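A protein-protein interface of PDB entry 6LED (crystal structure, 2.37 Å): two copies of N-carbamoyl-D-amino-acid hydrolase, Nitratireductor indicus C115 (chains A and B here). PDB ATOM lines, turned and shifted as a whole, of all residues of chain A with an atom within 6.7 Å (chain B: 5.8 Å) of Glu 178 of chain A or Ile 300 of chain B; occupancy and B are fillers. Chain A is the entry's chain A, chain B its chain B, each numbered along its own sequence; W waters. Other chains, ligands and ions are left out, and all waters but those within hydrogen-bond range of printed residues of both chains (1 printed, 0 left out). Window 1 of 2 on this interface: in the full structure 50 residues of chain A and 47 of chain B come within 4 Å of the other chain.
O of Ile 300 of chain B is in hydrogen-bond range of NH2 of Arg 292 of chain A (2.8 Å). NH2 of Arg 292 of chain A is in salt-bridge range of OE2 of Glu 178 of chain B (3.0 Å). The backbone carbonyl oxygen (O) of Gln 303 of chain B lies within hydrogen-bond range of the guanidinium group (NH1) of Arg 292 of chain A (2.8 Å). The guanidinium group (NH2) of Arg 292 of chain B sits at hydrogen-bond distance from the backbone carbonyl oxygen (O) of Ile 300 of chain A (2.8 Å). The side-chain hydroxyl (OG1) of Thr 301 of chain A sits at hydrogen-bond distance from the side-chain hydroxyl (OG1) of Thr 301 of chain B, at 2.9 Å. The backbone carbonyl oxygen (O) of Leu 185 of chain A lies within hydrogen-bond range of the side-chain amide nitrogen (NE2) of Gln 303 of chain B (3.4 Å). NE of Arg 181 of chain A is in salt-bridge range of OE2 of Glu 178 of chain B, 2.8 Å away. The side-chain carboxylate of Glu 178 of chain A is in salt-bridge range of the guanidinium group of Arg 181 of chain B, 2.8 Å away. The side-chain carboxylate (OE2) of Glu 178 of chain A lies within salt-bridge range of the guanidinium group (NH2) of Arg 292 of chain B, 3.0 Å away. The side-chain hydroxyl (OH) of Tyr 297 of chain B sits close to a ring nitrogen (NE2) of His 128 of chain A (2.4 Å).
OG1 of Thr 179 of chain A sits close to O of Trp 176 of chain A (3.4 Å). ND1 of His 128 of chain A lies within hydrogen-bond range of OD1 of Asp 173 of chain A (2.8 Å). O of Gln 298 of chain B sits at hydrogen-bond distance from OG of Ser 302 of chain B (2.8 Å). The guanidinium group of Arg 299 of chain B is in hydrogen-bond range of the side-chain amide oxygen of Gln 303 of chain B. O of Pro 294 of chain A is in hydrogen-bond range of NE2 of Gln 298 of chain A (2.9 Å). N of Arg 293 of chain A sits at hydrogen-bond distance from OH of Tyr 297 of chain A, 3.1 Å away.
Ile 300 of chain B touches Glu 178 of chain A. CA of Tyr 297 of chain B touches CG2 of Val 182 of chain A (3.96 Å). Arg 299 of chain B touches Leu 185 of chain A. Tyr 297 of chain A touches Glu 178 of chain B (CD1 to CB, 3.6 Å). CD2 of Tyr 297 of chain A touches O of Ile 300 of chain B (3.8 Å). Glu 178 of chain B touches Ile 300 of chain A. Arg 181 of chain B touches Ile 300 of chain A (CG to CG1, 3.9 Å). O of Ile 300 of chain A touches CD2 of Tyr 297 of chain B (3.7 Å). CD1 of Ile 300 of chain A touches CG2 of Ile 300 of chain B (3.9 Å). Gln 298 of chain B touches Thr 301 of chain A.
Printed residues of chain B within 4 Å of His 128 of chain A: Tyr 297. Of chain B, only Arg 181, Arg 292, Tyr 297 and Ile 300 come within 4 Å of Glu 178 of chain A. Of the printed residues of chain B, Arg 181 of chain A touches Glu 178 and Ile 300. The nearest printed residue of chain A that does not touch Ile 300 of chain B is Val 182 of chain A (4.02 Å).
Of the 21 printed residues of chain A, 13 touch a printed residue of chain B. Hydrophobic or aromatic side chains of chain A within 4 Å of the printed part of chain B: His 128, Trp 176, Val 177, Val 182, Leu 185, Pro 294, Tyr 297 and Ile 300. Among the printed residues, 31 pairs touch across the chains.
Arg 181 of chain A touches Ile 300 of chain B, and with the chains exchanged Ile 300 of chain A touches Arg 181 of chain B. Gln 298 of chain A touches Thr 301 of chain B, and with the chains exchanged Thr 301 of chain A touches Gln 298 of chain B. Ile 300 of chain A touches its own counterpart, Ile 300 of chain B. Thr 301 of chain A touches its own counterpart, Thr 301 of chain B. Of the 31 pairs that touch across the chains among the printed residues, 20 have their exchanged pair printed and touching as well.
Water W1 lies within hydrogen-bond range of O of Arg 175 of chain A (2.8 Å) and NH2 of Arg 181 of chain B (2.9 Å).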
ATOM      1  N   HIS A 128       5.580  -2.715  -5.407  1.00  0.00           N
ATOM      2  CA  HIS A 128       4.973  -2.406  -6.701  1.00  0.00           C
ATOM      3  C   HIS A 128       5.347  -0.980  -7.083  1.00  0.00           C
ATOM      4  O   HIS A 128       4.773  -0.015  -6.572  1.00  0.00           O
ATOM      5  CB  HIS A 128       3.461  -2.593  -6.648  1.00  0.00           C
ATOM      6  CG  HIS A 128       3.038  -3.962  -6.220  1.00  0.00           C
ATOM      7  ND1 HIS A 128       2.545  -4.232  -4.962  1.00  0.00           N
ATOM      8  CD2 HIS A 128       3.042  -5.143  -6.884  1.00  0.00           C
ATOM      9  CE1 HIS A 128       2.259  -5.518  -4.869  1.00  0.00           C
ATOM     10  NE2 HIS A 128       2.552  -6.094  -6.022  1.00  0.00           N
ATOM     11  N   PHE A 156       5.907  -7.952   2.414  1.00  0.00           N
ATOM     12  CA  PHE A 156       4.802  -7.375   3.181  1.00  0.00           C
ATOM     13  C   PHE A 156       4.847  -7.952   4.589  1.00  0.00           C
ATOM     14  O   PHE A 156       4.236  -8.980   4.885  1.00  0.00           O
ATOM     15  CB  PHE A 156       3.466  -7.658   2.506  1.00  0.00           C
ATOM     16  CG  PHE A 156       3.269  -6.928   1.210  1.00  0.00           C
ATOM     17  CD1 PHE A 156       3.147  -5.548   1.190  1.00  0.00           C
ATOM     18  CD2 PHE A 156       3.187  -7.620   0.013  1.00  0.00           C
ATOM     19  CE1 PHE A 156       2.959  -4.870   0.000  1.00  0.00           C
ATOM     20  CE2 PHE A 156       2.997  -6.950  -1.184  1.00  0.00           C
ATOM     21  CZ  PHE A 156       2.883  -5.573  -1.190  1.00  0.00           C
ATOM     22  N   ASP A 173       0.785   0.141  -3.962  1.00  0.00           N
ATOM     23  CA  ASP A 173       0.537  -1.178  -3.391  1.00  0.00           C
ATOM     24  C   ASP A 173      -0.945  -1.399  -3.117  1.00  0.00           C
ATOM     25  O   ASP A 173      -1.439  -2.524  -3.251  1.00  0.00           O
ATOM     26  CB  ASP A 173       1.327  -1.353  -2.092  1.00  0.00           C
ATOM     27  CG  ASP A 173       2.808  -1.557  -2.323  1.00  0.00           C
ATOM     28  OD1 ASP A 173       3.189  -2.049  -3.404  1.00  0.00           O
ATOM     29  OD2 ASP A 173       3.591  -1.228  -1.409  1.00  0.00           O
ATOM     30  N   ARG A 175      -3.533  -0.850  -4.700  1.00  0.00           N
ATOM     31  CA  ARG A 175      -4.354  -1.257  -5.832  1.00  0.00           C
ATOM     32  C   ARG A 175      -4.209  -2.734  -6.173  1.00  0.00           C
ATOM     33  O   ARG A 175      -4.960  -3.234  -7.019  1.00  0.00           O
ATOM     34  CB  ARG A 175      -4.009  -0.410  -7.063  1.00  0.00           C
ATOM     35  CG  ARG A 175      -4.124   1.082  -6.821  1.00  0.00           C
ATOM     36  CD  ARG A 175      -3.780   1.886  -8.062  1.00  0.00           C
ATOM     37  NE  ARG A 175      -3.755   3.317  -7.772  1.00  0.00           N
ATOM     38  CZ  ARG A 175      -4.828   4.100  -7.787  1.00  0.00           C
ATOM     39  NH1 ARG A 175      -4.711   5.390  -7.508  1.00  0.00           N
ATOM     40  NH2 ARG A 175      -6.018   3.593  -8.081  1.00  0.00           N
ATOM     41  N   TRP A 176      -3.273  -3.439  -5.542  1.00  0.00           N
ATOM     42  CA  TRP A 176      -3.039  -4.852  -5.805  1.00  0.00           C
ATOM     43  C   TRP A 176      -3.611  -5.686  -4.668  1.00  0.00           C
ATOM     44  O   TRP A 176      -3.325  -5.425  -3.495  1.00  0.00           O
ATOM     45  CB  TRP A 176      -1.543  -5.130  -5.975  1.00  0.00           C
ATOM     46  CG  TRP A 176      -0.939  -4.340  -7.088  1.00  0.00           C
ATOM     47  CD1 TRP A 176      -0.334  -3.121  -6.994  1.00  0.00           C
ATOM     48  CD2 TRP A 176      -0.897  -4.702  -8.473  1.00  0.00           C
ATOM     49  NE1 TRP A 176       0.089  -2.705  -8.233  1.00  0.00           N
ATOM     50  CE2 TRP A 176      -0.246  -3.658  -9.159  1.00  0.00           C
ATOM     51  CE3 TRP A 176      -1.344  -5.810  -9.199  1.00  0.00           C
ATOM     52  CZ2 TRP A 176      -0.034  -3.687 -10.534  1.00  0.00           C
ATOM     53  CZ3 TRP A 176      -1.133  -5.837 -10.564  1.00  0.00           C
ATOM     54  CH2 TRP A 176      -0.481  -4.783 -11.217  1.00  0.00           C
ATOM     55  N   VAL A 177      -4.420  -6.689  -5.019  1.00  0.00           N
ATOM     56  CA  VAL A 177      -5.056  -7.519  -4.000  1.00  0.00           C
ATOM     57  C   VAL A 177      -4.022  -8.334  -3.234  1.00  0.00           C
ATOM     58  O   VAL A 177      -4.235  -8.673  -2.063  1.00  0.00           O
ATOM     59  CB  VAL A 177      -6.128  -8.427  -4.637  1.00  0.00           C
ATOM     60  CG1 VAL A 177      -7.250  -7.589  -5.233  1.00  0.00           C
ATOM     61  CG2 VAL A 177      -5.509  -9.331  -5.694  1.00  0.00           C
ATOM     62  N   GLU A 178      -2.890  -8.657  -3.867  1.00  0.00           N
ATOM     63  CA  GLU A 178      -1.850  -9.420  -3.184  1.00  0.00           C
ATOM     64  C   GLU A 178      -1.301  -8.665  -1.982  1.00  0.00           C
ATOM     65  O   GLU A 178      -0.846  -9.285  -1.014  1.00  0.00           O
ATOM     66  CB  GLU A 178      -0.718  -9.761  -4.152  1.00  0.00           C
ATOM     67  CG  GLU A 178      -1.123 -10.656  -5.314  1.00  0.00           C
ATOM     68  CD  GLU A 178      -1.622  -9.875  -6.515  1.00  0.00           C
ATOM     69  OE1 GLU A 178      -1.997  -8.695  -6.348  1.00  0.00           O
ATOM     70  OE2 GLU A 178      -1.633 -10.442  -7.628  1.00  0.00           O
ATOM     71  N   THR A 179      -1.335  -7.330  -2.026  1.00  0.00           N
ATOM     72  CA  THR A 179      -0.860  -6.528  -0.904  1.00  0.00           C
ATOM     73  C   THR A 179      -1.633  -6.849   0.371  1.00  0.00           C
ATOM     74  O   THR A 179      -1.040  -7.155   1.412  1.00  0.00           O
ATOM     75  CB  THR A 179      -0.981  -5.041  -1.241  1.00  0.00           C
ATOM     76  OG1 THR A 179      -0.145  -4.731  -2.363  1.00  0.00           O
ATOM     77  CG2 THR A 179      -0.571  -4.191  -0.054  1.00  0.00           C
ATOM     78  N   TYR A 180      -2.965  -6.786   0.304  1.00  0.00           N
ATOM     79  CA  TYR A 180      -3.775  -7.026   1.494  1.00  0.00           C
ATOM     80  C   TYR A 180      -3.780  -8.502   1.875  1.00  0.00           C
ATOM     81  O   TYR A 180      -3.737  -8.840   3.064  1.00  0.00           O
ATOM     82  CB  TYR A 180      -5.206  -6.541   1.264  1.00  0.00           C
ATOM     83  CG  TYR A 180      -5.328  -5.118   0.770  1.00  0.00           C
ATOM     84  CD1 TYR A 180      -5.420  -4.057   1.664  1.00  0.00           C
ATOM     85  CD2 TYR A 180      -5.370  -4.836  -0.589  1.00  0.00           C
ATOM     86  CE1 TYR A 180      -5.540  -2.754   1.215  1.00  0.00           C
ATOM     87  CE2 TYR A 180      -5.492  -3.537  -1.048  1.00  0.00           C
ATOM     88  CZ  TYR A 180      -5.576  -2.500  -0.141  1.00  0.00           C
ATOM     89  OH  TYR A 180      -5.700  -1.207  -0.590  1.00  0.00           O
ATOM     90  N   ARG A 181      -3.837  -9.392   0.882  1.00  0.00           N
ATOM     91  CA  ARG A 181      -3.995 -10.814   1.172  1.00  0.00           C
ATOM     92  C   ARG A 181      -2.744 -11.396   1.822  1.00  0.00           C
ATOM     93  O   ARG A 181      -2.846 -12.219   2.740  1.00  0.00           O
ATOM     94  CB  ARG A 181      -4.347 -11.573  -0.107  1.00  0.00           C
ATOM     95  CG  ARG A 181      -4.479 -13.076   0.081  1.00  0.00           C
ATOM     96  CD  ARG A 181      -5.634 -13.443   1.005  1.00  0.00           C
ATOM     97  NE  ARG A 181      -6.880 -13.669   0.278  1.00  0.00           N
ATOM     98  CZ  ARG A 181      -8.010 -13.000   0.492  1.00  0.00           C
ATOM     99  NH1 ARG A 181      -8.063 -12.059   1.425  1.00  0.00           N
ATOM    100  NH2 ARG A 181      -9.093 -13.282  -0.222  1.00  0.00           N
ATOM    101  N   VAL A 182      -1.558 -10.985   1.365  1.00  0.00           N
ATOM    102  CA  VAL A 182      -0.320 -11.480   1.968  1.00  0.00           C
ATOM    103  C   VAL A 182      -0.275 -11.132   3.449  1.00  0.00           C
ATOM    104  O   VAL A 182       0.079 -11.967   4.290  1.00  0.00           O
ATOM    105  CB  VAL A 182       0.906 -10.927   1.216  1.00  0.00           C
ATOM    106  CG1 VAL A 182       2.161 -11.065   2.066  1.00  0.00           C
ATOM    107  CG2 VAL A 182       1.085 -11.655  -0.108  1.00  0.00           C
ATOM    108  N   MET A 183      -0.650  -9.900   3.795  1.00  0.00           N
ATOM    109  CA  MET A 183      -0.683  -9.509   5.197  1.00  0.00           C
ATOM    110  C   MET A 183      -1.896 -10.081   5.919  1.00  0.00           C
ATOM    111  O   MET A 183      -1.811 -10.388   7.113  1.00  0.00           O
ATOM    112  CB  MET A 183      -0.641  -7.983   5.308  1.00  0.00           C
ATOM    113  CG  MET A 183       0.679  -7.398   4.824  1.00  0.00           C
ATOM    114  SD  MET A 183       0.890  -5.630   5.113  1.00  0.00           S
ATOM    115  CE  MET A 183       0.016  -4.945   3.706  1.00  0.00           C
ATOM    116  N   GLY A 184      -3.020 -10.244   5.217  1.00  0.00           N
ATOM    117  CA  GLY A 184      -4.168 -10.901   5.826  1.00  0.00           C
ATOM    118  C   GLY A 184      -3.867 -12.332   6.226  1.00  0.00           C
ATOM    119  O   GLY A 184      -4.338 -12.813   7.261  1.00  0.00           O
ATOM    120  N   LEU A 185      -3.068 -13.030   5.418  1.00  0.00           N
ATOM    121  CA  LEU A 185      -2.597 -14.366   5.764  1.00  0.00           C
ATOM    122  C   LEU A 185      -1.593 -14.357   6.908  1.00  0.00           C
ATOM    123  O   LEU A 185      -1.175 -15.433   7.352  1.00  0.00           O
ATOM    124  CB  LEU A 185      -1.988 -15.033   4.531  1.00  0.00           C
ATOM    125  CG  LEU A 185      -2.996 -15.418   3.446  1.00  0.00           C
ATOM    126  CD1 LEU A 185      -2.291 -15.729   2.140  1.00  0.00           C
ATOM    127  CD2 LEU A 185      -3.835 -16.605   3.897  1.00  0.00           C
ATOM    128  N   ARG A 292     -10.261 -21.280   1.994  1.00  0.00           N
ATOM    129  CA  ARG A 292      -9.259 -21.079   0.955  1.00  0.00           C
ATOM    130  C   ARG A 292      -8.781 -22.412   0.388  1.00  0.00           C
ATOM    131  O   ARG A 292      -8.547 -23.375   1.124  1.00  0.00           O
ATOM    132  CB  ARG A 292      -8.078 -20.277   1.500  1.00  0.00           C
ATOM    133  CG  ARG A 292      -8.449 -18.854   1.902  1.00  0.00           C
ATOM    134  CD  ARG A 292      -7.230 -18.009   2.248  1.00  0.00           C
ATOM    135  NE  ARG A 292      -6.489 -17.583   1.063  1.00  0.00           N
ATOM    136  CZ  ARG A 292      -5.353 -18.138   0.650  1.00  0.00           C
ATOM    137  NH1 ARG A 292      -4.820 -19.145   1.329  1.00  0.00           N
ATOM    138  NH2 ARG A 292      -4.747 -17.682  -0.439  1.00  0.00           N
ATOM    139  N   ARG A 293      -8.646 -22.459  -0.939  1.00  0.00           N
ATOM    140  CA  ARG A 293      -8.207 -23.643  -1.674  1.00  0.00           C
ATOM    141  C   ARG A 293      -6.978 -23.256  -2.489  1.00  0.00           C
ATOM    142  O   ARG A 293      -7.085 -22.971  -3.692  1.00  0.00           O
ATOM    143  CB  ARG A 293      -9.315 -24.183  -2.576  1.00  0.00           C
ATOM    144  CG  ARG A 293     -10.660 -24.347  -1.890  1.00  0.00           C
ATOM    145  CD  ARG A 293     -10.629 -25.452  -0.849  1.00  0.00           C
ATOM    146  NE  ARG A 293     -10.221 -26.730  -1.423  1.00  0.00           N
ATOM    147  CZ  ARG A 293     -10.383 -27.904  -0.821  1.00  0.00           C
ATOM    148  NH1 ARG A 293     -10.957 -27.967   0.372  1.00  0.00           N
ATOM    149  NH2 ARG A 293      -9.980 -29.017  -1.418  1.00  0.00           N
ATOM    150  N   PRO A 294      -5.795 -23.241  -1.871  1.00  0.00           N
ATOM    151  CA  PRO A 294      -4.598 -22.753  -2.578  1.00  0.00           C
ATOM    152  C   PRO A 294      -4.191 -23.593  -3.781  1.00  0.00           C
ATOM    153  O   PRO A 294      -3.369 -23.125  -4.580  1.00  0.00           O
ATOM    154  CB  PRO A 294      -3.513 -22.776  -1.492  1.00  0.00           C
ATOM    155  CG  PRO A 294      -4.001 -23.768  -0.489  1.00  0.00           C
ATOM    156  CD  PRO A 294      -5.495 -23.643  -0.487  1.00  0.00           C
ATOM    157  N   TYR A 297      -4.897 -21.564  -6.904  1.00  0.00           N
ATOM    158  CA  TYR A 297      -4.388 -20.200  -6.976  1.00  0.00           C
ATOM    159  C   TYR A 297      -2.977 -20.130  -7.544  1.00  0.00           C
ATOM    160  O   TYR A 297      -2.351 -19.067  -7.486  1.00  0.00           O
ATOM    161  CB  TYR A 297      -4.406 -19.540  -5.592  1.00  0.00           C
ATOM    162  CG  TYR A 297      -5.702 -19.655  -4.812  1.00  0.00           C
ATOM    163  CD1 TYR A 297      -6.922 -19.837  -5.452  1.00  0.00           C
ATOM    164  CD2 TYR A 297      -5.700 -19.567  -3.425  1.00  0.00           C
ATOM    165  CE1 TYR A 297      -8.101 -19.944  -4.730  1.00  0.00           C
ATOM    166  CE2 TYR A 297      -6.870 -19.668  -2.697  1.00  0.00           C
ATOM    167  CZ  TYR A 297      -8.067 -19.855  -3.354  1.00  0.00           C
ATOM    168  OH  TYR A 297      -9.231 -19.957  -2.628  1.00  0.00           O
ATOM    169  N   GLN A 298      -2.469 -21.231  -8.107  1.00  0.00           N
ATOM    170  CA  GLN A 298      -1.044 -21.328  -8.413  1.00  0.00           C
ATOM    171  C   GLN A 298      -0.591 -20.289  -9.431  1.00  0.00           C
ATOM    172  O   GLN A 298       0.584 -19.903  -9.434  1.00  0.00           O
ATOM    173  CB  GLN A 298      -0.709 -22.734  -8.908  1.00  0.00           C
ATOM    174  CG  GLN A 298      -0.864 -23.804  -7.842  1.00  0.00           C
ATOM    175  CD  GLN A 298      -0.046 -23.504  -6.601  1.00  0.00           C
ATOM    176  OE1 GLN A 298       1.132 -23.156  -6.687  1.00  0.00           O
ATOM    177  NE2 GLN A 298      -0.672 -23.629  -5.435  1.00  0.00           N
ATOM    178  N   ILE A 300      -1.121 -17.242  -9.399  1.00  0.00           N
ATOM    179  CA  ILE A 300      -0.778 -15.995  -8.720  1.00  0.00           C
ATOM    180  C   ILE A 300       0.715 -15.925  -8.422  1.00  0.00           C
ATOM    181  O   ILE A 300       1.304 -14.837  -8.414  1.00  0.00           O
ATOM    182  CB  ILE A 300      -1.631 -15.845  -7.444  1.00  0.00           C
ATOM    183  CG1 ILE A 300      -3.117 -15.792  -7.811  1.00  0.00           C
ATOM    184  CG2 ILE A 300      -1.234 -14.602  -6.658  1.00  0.00           C
ATOM    185  CD1 ILE A 300      -4.040 -15.586  -6.631  1.00  0.00           C
ATOM    186  N   THR A 301       1.357 -17.072  -8.198  1.00  0.00           N
ATOM    187  CA  THR A 301       2.784 -17.109  -7.915  1.00  0.00           C
ATOM    188  C   THR A 301       3.611 -17.798  -8.993  1.00  0.00           C
ATOM    189  O   THR A 301       4.842 -17.699  -8.958  1.00  0.00           O
ATOM    190  CB  THR A 301       3.045 -17.802  -6.570  1.00  0.00           C
ATOM    191  OG1 THR A 301       2.422 -19.093  -6.565  1.00  0.00           O
ATOM    192  CG2 THR A 301       2.489 -16.971  -5.427  1.00  0.00           C
ATOM    193  N   GLU B 178      -8.707 -14.130  -5.041  1.00  0.00           N
ATOM    194  CA  GLU B 178      -8.032 -15.112  -5.882  1.00  0.00           C
ATOM    195  C   GLU B 178      -8.893 -15.516  -7.069  1.00  0.00           C
ATOM    196  O   GLU B 178      -8.363 -15.895  -8.120  1.00  0.00           O
ATOM    197  CB  GLU B 178      -7.656 -16.346  -5.059  1.00  0.00           C
ATOM    198  CG  GLU B 178      -6.643 -16.090  -3.948  1.00  0.00           C
ATOM    199  CD  GLU B 178      -7.282 -15.626  -2.649  1.00  0.00           C
ATOM    200  OE1 GLU B 178      -8.468 -15.233  -2.661  1.00  0.00           O
ATOM    201  OE2 GLU B 178      -6.593 -15.661  -1.609  1.00  0.00           O
ATOM    202  N   ARG B 181      -8.337 -12.770  -9.734  1.00  0.00           N
ATOM    203  CA  ARG B 181      -6.940 -12.655 -10.139  1.00  0.00           C
ATOM    204  C   ARG B 181      -6.494 -13.857 -10.963  1.00  0.00           C
ATOM    205  O   ARG B 181      -5.758 -13.701 -11.944  1.00  0.00           O
ATOM    206  CB  ARG B 181      -6.050 -12.480  -8.907  1.00  0.00           C
ATOM    207  CG  ARG B 181      -4.560 -12.430  -9.214  1.00  0.00           C
ATOM    208  CD  ARG B 181      -4.188 -11.237 -10.089  1.00  0.00           C
ATOM    209  NE  ARG B 181      -3.783 -10.071  -9.306  1.00  0.00           N
ATOM    210  CZ  ARG B 181      -4.470  -8.933  -9.234  1.00  0.00           C
ATOM    211  NH1 ARG B 181      -5.605  -8.793  -9.903  1.00  0.00           N
ATOM    212  NH2 ARG B 181      -4.014  -7.930  -8.495  1.00  0.00           N
ATOM    213  N   ARG B 292       3.823  -6.825 -11.376  1.00  0.00           N
ATOM    214  CA  ARG B 292       3.649  -7.860 -10.367  1.00  0.00           C
ATOM    215  C   ARG B 292       4.985  -8.480  -9.975  1.00  0.00           C
ATOM    216  O   ARG B 292       5.895  -8.623 -10.799  1.00  0.00           O
ATOM    217  CB  ARG B 292       2.686  -8.937 -10.868  1.00  0.00           C
ATOM    218  CG  ARG B 292       1.265  -8.426 -11.073  1.00  0.00           C
ATOM    219  CD  ARG B 292       0.285  -9.539 -11.419  1.00  0.00           C
ATOM    220  NE  ARG B 292      -0.005 -10.400 -10.276  1.00  0.00           N
ATOM    221  CZ  ARG B 292       0.497 -11.621 -10.110  1.00  0.00           C
ATOM    222  NH1 ARG B 292       1.316 -12.135 -11.018  1.00  0.00           N
ATOM    223  NH2 ARG B 292       0.173 -12.329  -9.036  1.00  0.00           N
ATOM    224  N   TYR B 297       4.446 -13.057  -3.121  1.00  0.00           N
ATOM    225  CA  TYR B 297       3.065 -13.507  -2.993  1.00  0.00           C
ATOM    226  C   TYR B 297       2.958 -14.956  -2.535  1.00  0.00           C
ATOM    227  O   TYR B 297       1.869 -15.536  -2.609  1.00  0.00           O
ATOM    228  CB  TYR B 297       2.318 -13.348  -4.323  1.00  0.00           C
ATOM    229  CG  TYR B 297       2.422 -11.995  -5.001  1.00  0.00           C
ATOM    230  CD1 TYR B 297       2.720 -10.841  -4.285  1.00  0.00           C
ATOM    231  CD2 TYR B 297       2.201 -11.877  -6.367  1.00  0.00           C
ATOM    232  CE1 TYR B 297       2.807  -9.612  -4.918  1.00  0.00           C
ATOM    233  CE2 TYR B 297       2.288 -10.657  -7.006  1.00  0.00           C
ATOM    234  CZ  TYR B 297       2.589  -9.528  -6.280  1.00  0.00           C
ATOM    235  OH  TYR B 297       2.672  -8.314  -6.924  1.00  0.00           O
ATOM    236  N   GLN B 298       4.055 -15.552  -2.058  1.00  0.00           N
ATOM    237  CA  GLN B 298       4.093 -17.002  -1.870  1.00  0.00           C
ATOM    238  C   GLN B 298       3.102 -17.481  -0.816  1.00  0.00           C
ATOM    239  O   GLN B 298       2.620 -18.617  -0.898  1.00  0.00           O
ATOM    240  CB  GLN B 298       5.509 -17.448  -1.504  1.00  0.00           C
ATOM    241  CG  GLN B 298       6.527 -17.223  -2.611  1.00  0.00           C
ATOM    242  CD  GLN B 298       6.148 -17.918  -3.906  1.00  0.00           C
ATOM    243  OE1 GLN B 298       5.687 -19.060  -3.901  1.00  0.00           O
ATOM    244  NE2 GLN B 298       6.334 -17.226  -5.025  1.00  0.00           N
ATOM    245  N   ARG B 299       2.784 -16.646   0.176  1.00  0.00           N
ATOM    246  CA  ARG B 299       1.828 -17.060   1.200  1.00  0.00           C
ATOM    247  C   ARG B 299       0.458 -17.359   0.604  1.00  0.00           C
ATOM    248  O   ARG B 299      -0.280 -18.194   1.139  1.00  0.00           O
ATOM    249  CB  ARG B 299       1.708 -15.987   2.282  1.00  0.00           C
ATOM    250  CG  ARG B 299       2.909 -15.886   3.206  1.00  0.00           C
ATOM    251  CD  ARG B 299       2.680 -14.829   4.273  1.00  0.00           C
ATOM    252  NE  ARG B 299       3.831 -14.674   5.156  1.00  0.00           N
ATOM    253  CZ  ARG B 299       3.984 -15.321   6.308  1.00  0.00           C
ATOM    254  NH1 ARG B 299       5.063 -15.114   7.047  1.00  0.00           N
ATOM    255  NH2 ARG B 299       3.055 -16.174   6.721  1.00  0.00           N
ATOM    256  N   ILE B 300       0.106 -16.698  -0.501  1.00  0.00           N
ATOM    257  CA  ILE B 300      -1.206 -16.893  -1.109  1.00  0.00           C
ATOM    258  C   ILE B 300      -1.370 -18.321  -1.615  1.00  0.00           C
ATOM    259  O   ILE B 300      -2.467 -18.890  -1.549  1.00  0.00           O
ATOM    260  CB  ILE B 300      -1.421 -15.858  -2.233  1.00  0.00           C
ATOM    261  CG1 ILE B 300      -1.367 -14.438  -1.661  1.00  0.00           C
ATOM    262  CG2 ILE B 300      -2.743 -16.093  -2.947  1.00  0.00           C
ATOM    263  CD1 ILE B 300      -1.534 -13.349  -2.700  1.00  0.00           C
ATOM    264  N   THR B 301      -0.293 -18.932  -2.103  1.00  0.00           N
ATOM    265  CA  THR B 301      -0.354 -20.277  -2.656  1.00  0.00           C
ATOM    266  C   THR B 301       0.288 -21.328  -1.762  1.00  0.00           C
ATOM    267  O   THR B 301       0.223 -22.518  -2.088  1.00  0.00           O
ATOM    268  CB  THR B 301       0.304 -20.308  -4.040  1.00  0.00           C
ATOM    269  OG1 THR B 301       1.680 -19.922  -3.928  1.00  0.00           O
ATOM    270  CG2 THR B 301      -0.405 -19.349  -4.980  1.00  0.00           C
ATOM    271  N   SER B 302       0.897 -20.931  -0.645  1.00  0.00           N
ATOM    272  CA  SER B 302       1.542 -21.891   0.243  1.00  0.00           C
ATOM    273  C   SER B 302       0.618 -22.346   1.367  1.00  0.00           C
ATOM    274  O   SER B 302       0.435 -23.551   1.574  1.00  0.00           O
ATOM    275  CB  SER B 302       2.823 -21.290   0.832  1.00  0.00           C
ATOM    276  OG  SER B 302       3.785 -21.047  -0.181  1.00  0.00           O
ATOM    277  N   GLN B 303       0.030 -21.404   2.095  1.00  0.00           N
ATOM    278  CA  GLN B 303      -0.775 -21.707   3.267  1.00  0.00           C
ATOM    279  C   GLN B 303      -2.252 -21.448   2.997  1.00  0.00           C
ATOM    280  O   GLN B 303      -2.628 -20.752   2.049  1.00  0.00           O
ATOM    281  CB  GLN B 303      -0.315 -20.879   4.472  1.00  0.00           C
ATOM    282  CG  GLN B 303      -0.236 -19.386   4.204  1.00  0.00           C
ATOM    283  CD  GLN B 303       0.182 -18.597   5.428  1.00  0.00           C
ATOM    284  OE1 GLN B 303       1.231 -17.953   5.439  1.00  0.00           O
ATOM    285  NE2 GLN B 303      -0.641 -18.640   6.468  1.00  0.00           N
HETATM  286  O   HOH W   1      -5.110  -5.236  -8.947  1.00  0.00           O
